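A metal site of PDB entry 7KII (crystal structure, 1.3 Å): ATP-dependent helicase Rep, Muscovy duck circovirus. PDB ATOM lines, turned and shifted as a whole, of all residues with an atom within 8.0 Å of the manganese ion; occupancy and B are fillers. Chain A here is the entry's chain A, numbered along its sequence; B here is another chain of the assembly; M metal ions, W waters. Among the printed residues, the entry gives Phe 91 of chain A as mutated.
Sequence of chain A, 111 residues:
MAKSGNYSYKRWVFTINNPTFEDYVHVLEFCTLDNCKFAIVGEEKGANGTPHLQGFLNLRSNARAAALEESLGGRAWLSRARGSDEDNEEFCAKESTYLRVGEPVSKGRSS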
ATOM      1  N   PHE A  14     -16.823  16.231 -17.564  1.00  0.00           N
ATOM      2  CA  PHE A  14     -17.697  16.051 -18.708  1.00  0.00           C
ATOM      3  C   PHE A  14     -18.359  14.678 -18.678  1.00  0.00           C
ATOM      4  O   PHE A  14     -17.850  13.740 -18.055  1.00  0.00           O
ATOM      5  CB  PHE A  14     -16.995  16.337 -20.056  1.00  0.00           C
ATOM      6  CG  PHE A  14     -16.010  15.268 -20.500  1.00  0.00           C
ATOM      7  CD1 PHE A  14     -16.430  14.179 -21.243  1.00  0.00           C
ATOM      8  CD2 PHE A  14     -14.656  15.407 -20.224  1.00  0.00           C
ATOM      9  CE1 PHE A  14     -15.515  13.222 -21.664  1.00  0.00           C
ATOM     10  CE2 PHE A  14     -13.735  14.449 -20.657  1.00  0.00           C
ATOM     11  CZ  PHE A  14     -14.177  13.365 -21.372  1.00  0.00           C
ATOM     12  N   THR A  15     -19.503  14.599 -19.350  1.00  0.00           N
ATOM     13  CA  THR A  15     -20.206  13.355 -19.610  1.00  0.00           C
ATOM     14  C   THR A  15     -20.593  13.323 -21.081  1.00  0.00           C
ATOM     15  O   THR A  15     -21.057  14.331 -21.627  1.00  0.00           O
ATOM     16  CB  THR A  15     -21.520  13.276 -18.787  1.00  0.00           C
ATOM     17  OG1 THR A  15     -21.221  13.437 -17.392  1.00  0.00           O
ATOM     18  CG2 THR A  15     -22.238  11.943 -19.020  1.00  0.00           C
ATOM     19  N   ASN A  17     -23.121  10.946 -23.103  1.00  0.00           N
ATOM     20  CA  ASN A  17     -24.075   9.842 -23.124  1.00  0.00           C
ATOM     21  C   ASN A  17     -24.206   9.270 -24.528  1.00  0.00           C
ATOM     22  O   ASN A  17     -24.195  10.005 -25.511  1.00  0.00           O
ATOM     23  CB  ASN A  17     -25.445  10.332 -22.638  1.00  0.00           C
ATOM     24  CG  ASN A  17     -25.529  10.350 -21.127  1.00  0.00           C
ATOM     25  OD1 ASN A  17     -25.372   9.323 -20.477  1.00  0.00           O
ATOM     26  ND2 ASN A  17     -25.741  11.545 -20.566  1.00  0.00           N
ATOM     27  N   GLY A  42     -13.675   7.354 -18.067  1.00  0.00           N
ATOM     28  CA  GLY A  42     -14.173   5.996 -17.855  1.00  0.00           C
ATOM     29  C   GLY A  42     -15.396   5.713 -18.722  1.00  0.00           C
ATOM     30  O   GLY A  42     -16.250   6.576 -18.918  1.00  0.00           O
ATOM     31  N   GLU A  43     -15.476   4.484 -19.217  1.00  0.00           N
ATOM     32  CA  GLU A  43     -16.678   4.017 -19.908  1.00  0.00           C
ATOM     33  C   GLU A  43     -17.595   3.379 -18.875  1.00  0.00           C
ATOM     34  O   GLU A  43     -17.195   2.450 -18.164  1.00  0.00           O
ATOM     35  CB  GLU A  43     -16.284   3.006 -20.982  1.00  0.00           C
ATOM     36  CG  GLU A  43     -17.364   2.757 -22.006  1.00  0.00           C
ATOM     37  CD  GLU A  43     -16.989   1.667 -22.976  1.00  0.00           C
ATOM     38  OE1 GLU A  43     -17.303   1.809 -24.179  1.00  0.00           O
ATOM     39  OE2 GLU A  43     -16.388   0.664 -22.546  1.00  0.00           O
ATOM     40  N   GLU A  44     -18.824   3.897 -18.767  1.00  0.00           N
ATOM     41  CA  GLU A  44     -19.682   3.553 -17.639  1.00  0.00           C
ATOM     42  C   GLU A  44     -21.120   3.305 -18.078  1.00  0.00           C
ATOM     43  O   GLU A  44     -21.533   3.650 -19.188  1.00  0.00           O
ATOM     44  CB  GLU A  44     -19.685   4.685 -16.602  1.00  0.00           C
ATOM     45  CG  GLU A  44     -18.324   4.963 -15.999  1.00  0.00           C
ATOM     46  CD  GLU A  44     -18.387   5.860 -14.787  1.00  0.00           C
ATOM     47  OE1 GLU A  44     -19.333   6.673 -14.697  1.00  0.00           O
ATOM     48  OE2 GLU A  44     -17.504   5.739 -13.917  1.00  0.00           O
ATOM     49  N   LYS A  45     -21.874   2.695 -17.166  1.00  0.00           N
ATOM     50  CA  LYS A  45     -23.321   2.601 -17.239  1.00  0.00           C
ATOM     51  C   LYS A  45     -23.868   2.863 -15.844  1.00  0.00           C
ATOM     52  O   LYS A  45     -23.328   2.349 -14.863  1.00  0.00           O
ATOM     53  CB  LYS A  45     -23.782   1.198 -17.654  1.00  0.00           C
ATOM     54  CG  LYS A  45     -23.653   0.897 -19.123  1.00  0.00           C
ATOM     55  CD  LYS A  45     -24.212  -0.501 -19.443  1.00  0.00           C
ATOM     56  CE  LYS A  45     -24.268  -0.739 -20.932  1.00  0.00           C
ATOM     57  NZ  LYS A  45     -24.490  -2.189 -21.246  1.00  0.00           N
ATOM     58  N   GLY A  46     -24.931   3.657 -15.761  1.00  0.00           N
ATOM     59  CA  GLY A  46     -25.643   3.862 -14.520  1.00  0.00           C
ATOM     60  C   GLY A  46     -26.812   2.910 -14.396  1.00  0.00           C
ATOM     61  O   GLY A  46     -26.897   1.882 -15.069  1.00  0.00           O
ATOM     62  N   ALA A  47     -27.753   3.277 -13.509  1.00  0.00           N
ATOM     63  CA  ALA A  47     -28.903   2.421 -13.245  1.00  0.00           C
ATOM     64  C   ALA A  47     -29.756   2.195 -14.484  1.00  0.00           C
ATOM     65  O   ALA A  47     -30.326   1.110 -14.644  1.00  0.00           O
ATOM     66  CB  ALA A  47     -29.742   3.006 -12.106  1.00  0.00           C
ATOM     67  N   THR A  50     -27.550   3.338 -19.563  1.00  0.00           N
ATOM     68  CA  THR A  50     -27.152   4.174 -20.678  1.00  0.00           C
ATOM     69  C   THR A  50     -25.634   4.259 -20.712  1.00  0.00           C
ATOM     70  O   THR A  50     -25.030   4.776 -19.766  1.00  0.00           O
ATOM     71  CB  THR A  50     -27.753   5.565 -20.555  1.00  0.00           C
ATOM     72  OG1 THR A  50     -29.182   5.444 -20.552  1.00  0.00           O
ATOM     73  CG2 THR A  50     -27.328   6.425 -21.739  1.00  0.00           C
ATOM     74  N   PRO A  51     -24.973   3.744 -21.757  1.00  0.00           N
ATOM     75  CA  PRO A  51     -23.513   3.836 -21.804  1.00  0.00           C
ATOM     76  C   PRO A  51     -23.100   5.290 -21.927  1.00  0.00           C
ATOM     77  O   PRO A  51     -23.733   6.076 -22.631  1.00  0.00           O
ATOM     78  CB  PRO A  51     -23.152   3.053 -23.066  1.00  0.00           C
ATOM     79  CG  PRO A  51     -24.351   3.169 -23.932  1.00  0.00           C
ATOM     80  CD  PRO A  51     -25.544   3.200 -23.000  1.00  0.00           C
ATOM     81  N   HIS A  52     -22.026   5.647 -21.238  1.00  0.00           N
ATOM     82  CA  HIS A  52     -21.566   7.025 -21.257  1.00  0.00           C
ATOM     83  C   HIS A  52     -20.099   7.079 -20.899  1.00  0.00           C
ATOM     84  O   HIS A  52     -19.562   6.185 -20.228  1.00  0.00           O
ATOM     85  CB  HIS A  52     -22.417   7.916 -20.336  1.00  0.00           C
ATOM     86  CG  HIS A  52     -22.384   7.528 -18.891  1.00  0.00           C
ATOM     87  ND1 HIS A  52     -23.131   6.485 -18.381  1.00  0.00           N
ATOM     88  CD2 HIS A  52     -21.726   8.060 -17.834  1.00  0.00           C
ATOM     89  CE1 HIS A  52     -22.925   6.382 -17.077  1.00  0.00           C
ATOM     90  NE2 HIS A  52     -22.074   7.335 -16.723  1.00  0.00           N
ATOM     91  N   LEU A  53     -19.446   8.138 -21.377  1.00  0.00           N
ATOM     92  CA  LEU A  53     -18.088   8.450 -20.971  1.00  0.00           C
ATOM     93  C   LEU A  53     -18.165   9.414 -19.790  1.00  0.00           C
ATOM     94  O   LEU A  53     -18.934  10.387 -19.823  1.00  0.00           O
ATOM     95  CB  LEU A  53     -17.312   9.087 -22.129  1.00  0.00           C
ATOM     96  CG  LEU A  53     -17.246   8.190 -23.363  1.00  0.00           C
ATOM     97  CD1 LEU A  53     -16.407   8.829 -24.466  1.00  0.00           C
ATOM     98  CD2 LEU A  53     -16.710   6.801 -23.003  1.00  0.00           C
ATOM     99  N   GLN A  54     -17.392   9.125 -18.755  1.00  0.00           N
ATOM    100  CA  GLN A  54     -17.360   9.891 -17.511  1.00  0.00           C
ATOM    101  C   GLN A  54     -15.954  10.453 -17.390  1.00  0.00           C
ATOM    102  O   GLN A  54     -14.995   9.706 -17.141  1.00  0.00           O
ATOM    103  CB  GLN A  54     -17.683   8.951 -16.346  1.00  0.00           C
ATOM    104  CG  GLN A  54     -18.132   9.675 -15.104  1.00  0.00           C
ATOM    105  CD  GLN A  54     -19.508  10.258 -15.291  1.00  0.00           C
ATOM    106  OE1 GLN A  54     -20.483   9.514 -15.439  1.00  0.00           O
ATOM    107  NE2 GLN A  54     -19.602  11.593 -15.300  1.00  0.00           N
ATOM    108  N   GLY A  55     -15.801  11.773 -17.561  1.00  0.00           N
ATOM    109  CA  GLY A  55     -14.498  12.346 -17.785  1.00  0.00           C
ATOM    110  C   GLY A  55     -14.150  13.495 -16.855  1.00  0.00           C
ATOM    111  O   GLY A  55     -15.018  14.209 -16.325  1.00  0.00           O
ATOM    112  N   PHE A  91     -13.385   8.908  -9.000  1.00  0.00           N
ATOM    113  CA  PHE A  91     -14.753   8.828  -9.496  1.00  0.00           C
ATOM    114  C   PHE A  91     -14.797   8.285 -10.925  1.00  0.00           C
ATOM    115  O   PHE A  91     -15.668   7.472 -11.258  1.00  0.00           O
ATOM    116  CB  PHE A  91     -15.428  10.188  -9.405  1.00  0.00           C
ATOM    117  CG  PHE A  91     -16.905  10.125  -9.656  1.00  0.00           C
ATOM    118  CD1 PHE A  91     -17.432  10.493 -10.897  1.00  0.00           C
ATOM    119  CD2 PHE A  91     -17.774   9.682  -8.671  1.00  0.00           C
ATOM    120  CE1 PHE A  91     -18.797  10.420 -11.131  1.00  0.00           C
ATOM    121  CE2 PHE A  91     -19.142   9.599  -8.905  1.00  0.00           C
ATOM    122  CZ  PHE A  91     -19.650   9.972 -10.130  1.00  0.00           C
ATOM    123  N   CYS A  92     -13.876   8.733 -11.789  1.00  0.00           N
ATOM    124  CA  CYS A  92     -13.927   8.316 -13.181  1.00  0.00           C
ATOM    125  C   CYS A  92     -13.298   6.939 -13.428  1.00  0.00           C
ATOM    126  O   CYS A  92     -13.448   6.401 -14.528  1.00  0.00           O
ATOM    127  CB  CYS A  92     -13.330   9.375 -14.116  1.00  0.00           C
ATOM    128  SG  CYS A  92     -14.226  10.932 -14.094  1.00  0.00           S
ATOM    129  N   LYS A  94     -14.097   4.347 -11.360  1.00  0.00           N
ATOM    130  CA  LYS A  94     -14.840   3.454 -10.479  1.00  0.00           C
ATOM    131  C   LYS A  94     -15.435   2.236 -11.181  1.00  0.00           C
ATOM    132  O   LYS A  94     -15.763   1.251 -10.512  1.00  0.00           O
ATOM    133  CB  LYS A  94     -15.938   4.219  -9.736  1.00  0.00           C
ATOM    134  CG  LYS A  94     -17.081   4.682 -10.618  1.00  0.00           C
ATOM    135  CD  LYS A  94     -18.036   5.595  -9.862  1.00  0.00           C
ATOM    136  CE  LYS A  94     -19.124   6.136 -10.775  1.00  0.00           C
ATOM    137  NZ  LYS A  94     -18.538   7.156 -11.710  1.00  0.00           N
ATOM    138  N   GLU A  95     -15.602   2.266 -12.504  1.00  0.00           N
ATOM    139  CA  GLU A  95     -16.150   1.108 -13.214  1.00  0.00           C
ATOM    140  C   GLU A  95     -15.091   0.344 -14.008  1.00  0.00           C
ATOM    141  O   GLU A  95     -15.433  -0.570 -14.759  1.00  0.00           O
ATOM    142  CB  GLU A  95     -17.368   1.488 -14.060  1.00  0.00           C
ATOM    143  CG  GLU A  95     -18.529   2.020 -13.183  1.00  0.00           C
ATOM    144  CD  GLU A  95     -19.764   2.425 -13.968  1.00  0.00           C
ATOM    145  OE1 GLU A  95     -20.473   3.355 -13.498  1.00  0.00           O
ATOM    146  OE2 GLU A  95     -20.038   1.817 -15.026  1.00  0.00           O
ATOM    147  P    DT B   7     -28.303   6.645 -14.165  1.00  0.00           P
ATOM    148  OP1  DT B   7     -28.808   5.728 -15.202  1.00  0.00           O
ATOM    149  OP2  DT B   7     -28.114   6.121 -12.792  1.00  0.00           O
ATOM    150  O5'  DT B   7     -26.933   7.204 -14.727  1.00  0.00           O
ATOM    151  C5'  DT B   7     -26.175   8.137 -13.989  1.00  0.00           C
ATOM    152  C4'  DT B   7     -25.129   8.758 -14.885  1.00  0.00           C
ATOM    153  O4'  DT B   7     -25.790   9.556 -15.905  1.00  0.00           O
ATOM    154  C3'  DT B   7     -24.154   9.683 -14.173  1.00  0.00           C
ATOM    155  O3'  DT B   7     -23.002   8.933 -13.837  1.00  0.00           O
ATOM    156  C2'  DT B   7     -23.843  10.760 -15.227  1.00  0.00           C
ATOM    157  C1'  DT B   7     -25.100  10.788 -16.095  1.00  0.00           C
ATOM    158  N1   DT B   7     -26.070  11.875 -15.749  1.00  0.00           N
ATOM    159  C2   DT B   7     -26.854  12.395 -16.748  1.00  0.00           C
ATOM    160  O2   DT B   7     -26.757  12.069 -17.904  1.00  0.00           O
ATOM    161  N3   DT B   7     -27.747  13.335 -16.346  1.00  0.00           N
ATOM    162  C4   DT B   7     -27.964  13.786 -15.066  1.00  0.00           C
ATOM    163  O4   DT B   7     -28.810  14.632 -14.804  1.00  0.00           O
ATOM    164  C5   DT B   7     -27.132  13.180 -14.049  1.00  0.00           C
ATOM    165  C7   DT B   7     -27.286  13.591 -12.614  1.00  0.00           C
ATOM    166  C6   DT B   7     -26.243  12.251 -14.438  1.00  0.00           C
ATOM    167  P    DA B   8     -22.150   9.252 -12.514  1.00  0.00           P
ATOM    168  OP1  DA B   8     -20.966   8.362 -12.644  1.00  0.00           O
ATOM    169  OP2  DA B   8     -23.006   9.155 -11.321  1.00  0.00           O
ATOM    170  O5'  DA B   8     -21.668  10.739 -12.751  1.00  0.00           O
ATOM    171  C5'  DA B   8     -22.165  11.825 -11.974  1.00  0.00           C
ATOM    172  C4'  DA B   8     -21.606  13.098 -12.581  1.00  0.00           C
ATOM    173  O4'  DA B   8     -22.267  13.347 -13.834  1.00  0.00           O
ATOM    174  C3'  DA B   8     -21.820  14.363 -11.792  1.00  0.00           C
ATOM    175  O3'  DA B   8     -20.867  14.471 -10.773  1.00  0.00           O
ATOM    176  C2'  DA B   8     -21.565  15.394 -12.875  1.00  0.00           C
ATOM    177  C1'  DA B   8     -22.216  14.727 -14.094  1.00  0.00           C
ATOM    178  N9   DA B   8     -23.533  15.306 -14.427  1.00  0.00           N
ATOM    179  C8   DA B   8     -24.310  16.105 -13.633  1.00  0.00           C
ATOM    180  N7   DA B   8     -25.382  16.556 -14.233  1.00  0.00           N
ATOM    181  C5   DA B   8     -25.287  16.055 -15.511  1.00  0.00           C
ATOM    182  C6   DA B   8     -26.116  16.174 -16.640  1.00  0.00           C
ATOM    183  N6   DA B   8     -27.216  16.928 -16.665  1.00  0.00           N
ATOM    184  N1   DA B   8     -25.734  15.551 -17.777  1.00  0.00           N
ATOM    185  C2   DA B   8     -24.618  14.824 -17.754  1.00  0.00           C
ATOM    186  N3   DA B   8     -23.763  14.627 -16.746  1.00  0.00           N
ATOM    187  C4   DA B   8     -24.161  15.286 -15.653  1.00  0.00           C
HETATM  188 MN    MN M   1     -21.161   7.547 -14.747  1.00  0.00          MN
HETATM  189  O   HOH W   1     -22.378   5.624 -13.945  1.00  0.00           O
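The side-chain hydroxyl (OG1) of Thr 15 sits at hydrogen-bond distance from the side-chain amide nitrogen (NE2) of Gln 54. The backbone NH (N) of Gln 54 lies within hydrogen-bond range of the backbone carbonyl oxygen (O) of Gly 42, at 2.8 Å. O2 of DT 7 of chain B lies within hydrogen-bond range of the side-chain amide nitrogen of Asn 17 (2.9 Å). The side-chain carboxylate of Glu 44 lies within salt-bridge range of the side-chain amino group of Lys 94 (2.8 Å). The backbone carbonyl oxygen of Gln 54 is in hydrogen-bond range of the side-chain sulfur of Cys 92, 3.4 Å away. OP1 of DA 8 of chain B lies close to the side-chain amino group of Lys 94, 2.9 Å away. A ring nitrogen (ND1) of His 52 sits at hydrogen-bond distance from the backbone carbonyl oxygen (O) of Thr 50. OG1 of Thr 15 sits at hydrogen-bond distance from N3 of DA 8 of chain B (2.9 Å).
Of the 21 residues printed, 5 come within 4 Å of the manganese ion. Along chain A the residues within 4 Å of the manganese ion span positions 44 to 54. The nearest printed residue that does not touch the manganese ion is Lys 94 (4.03 Å).
The manganese ion is bound by the side-chain carboxylate (OE1) of Glu 44, a ring nitrogen (NE2) of His 52, the side-chain amide oxygen (OE1) of Gln 54, OP1 of DA 8 of chain B, water W1 and O3' of DT 7 of chain B.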
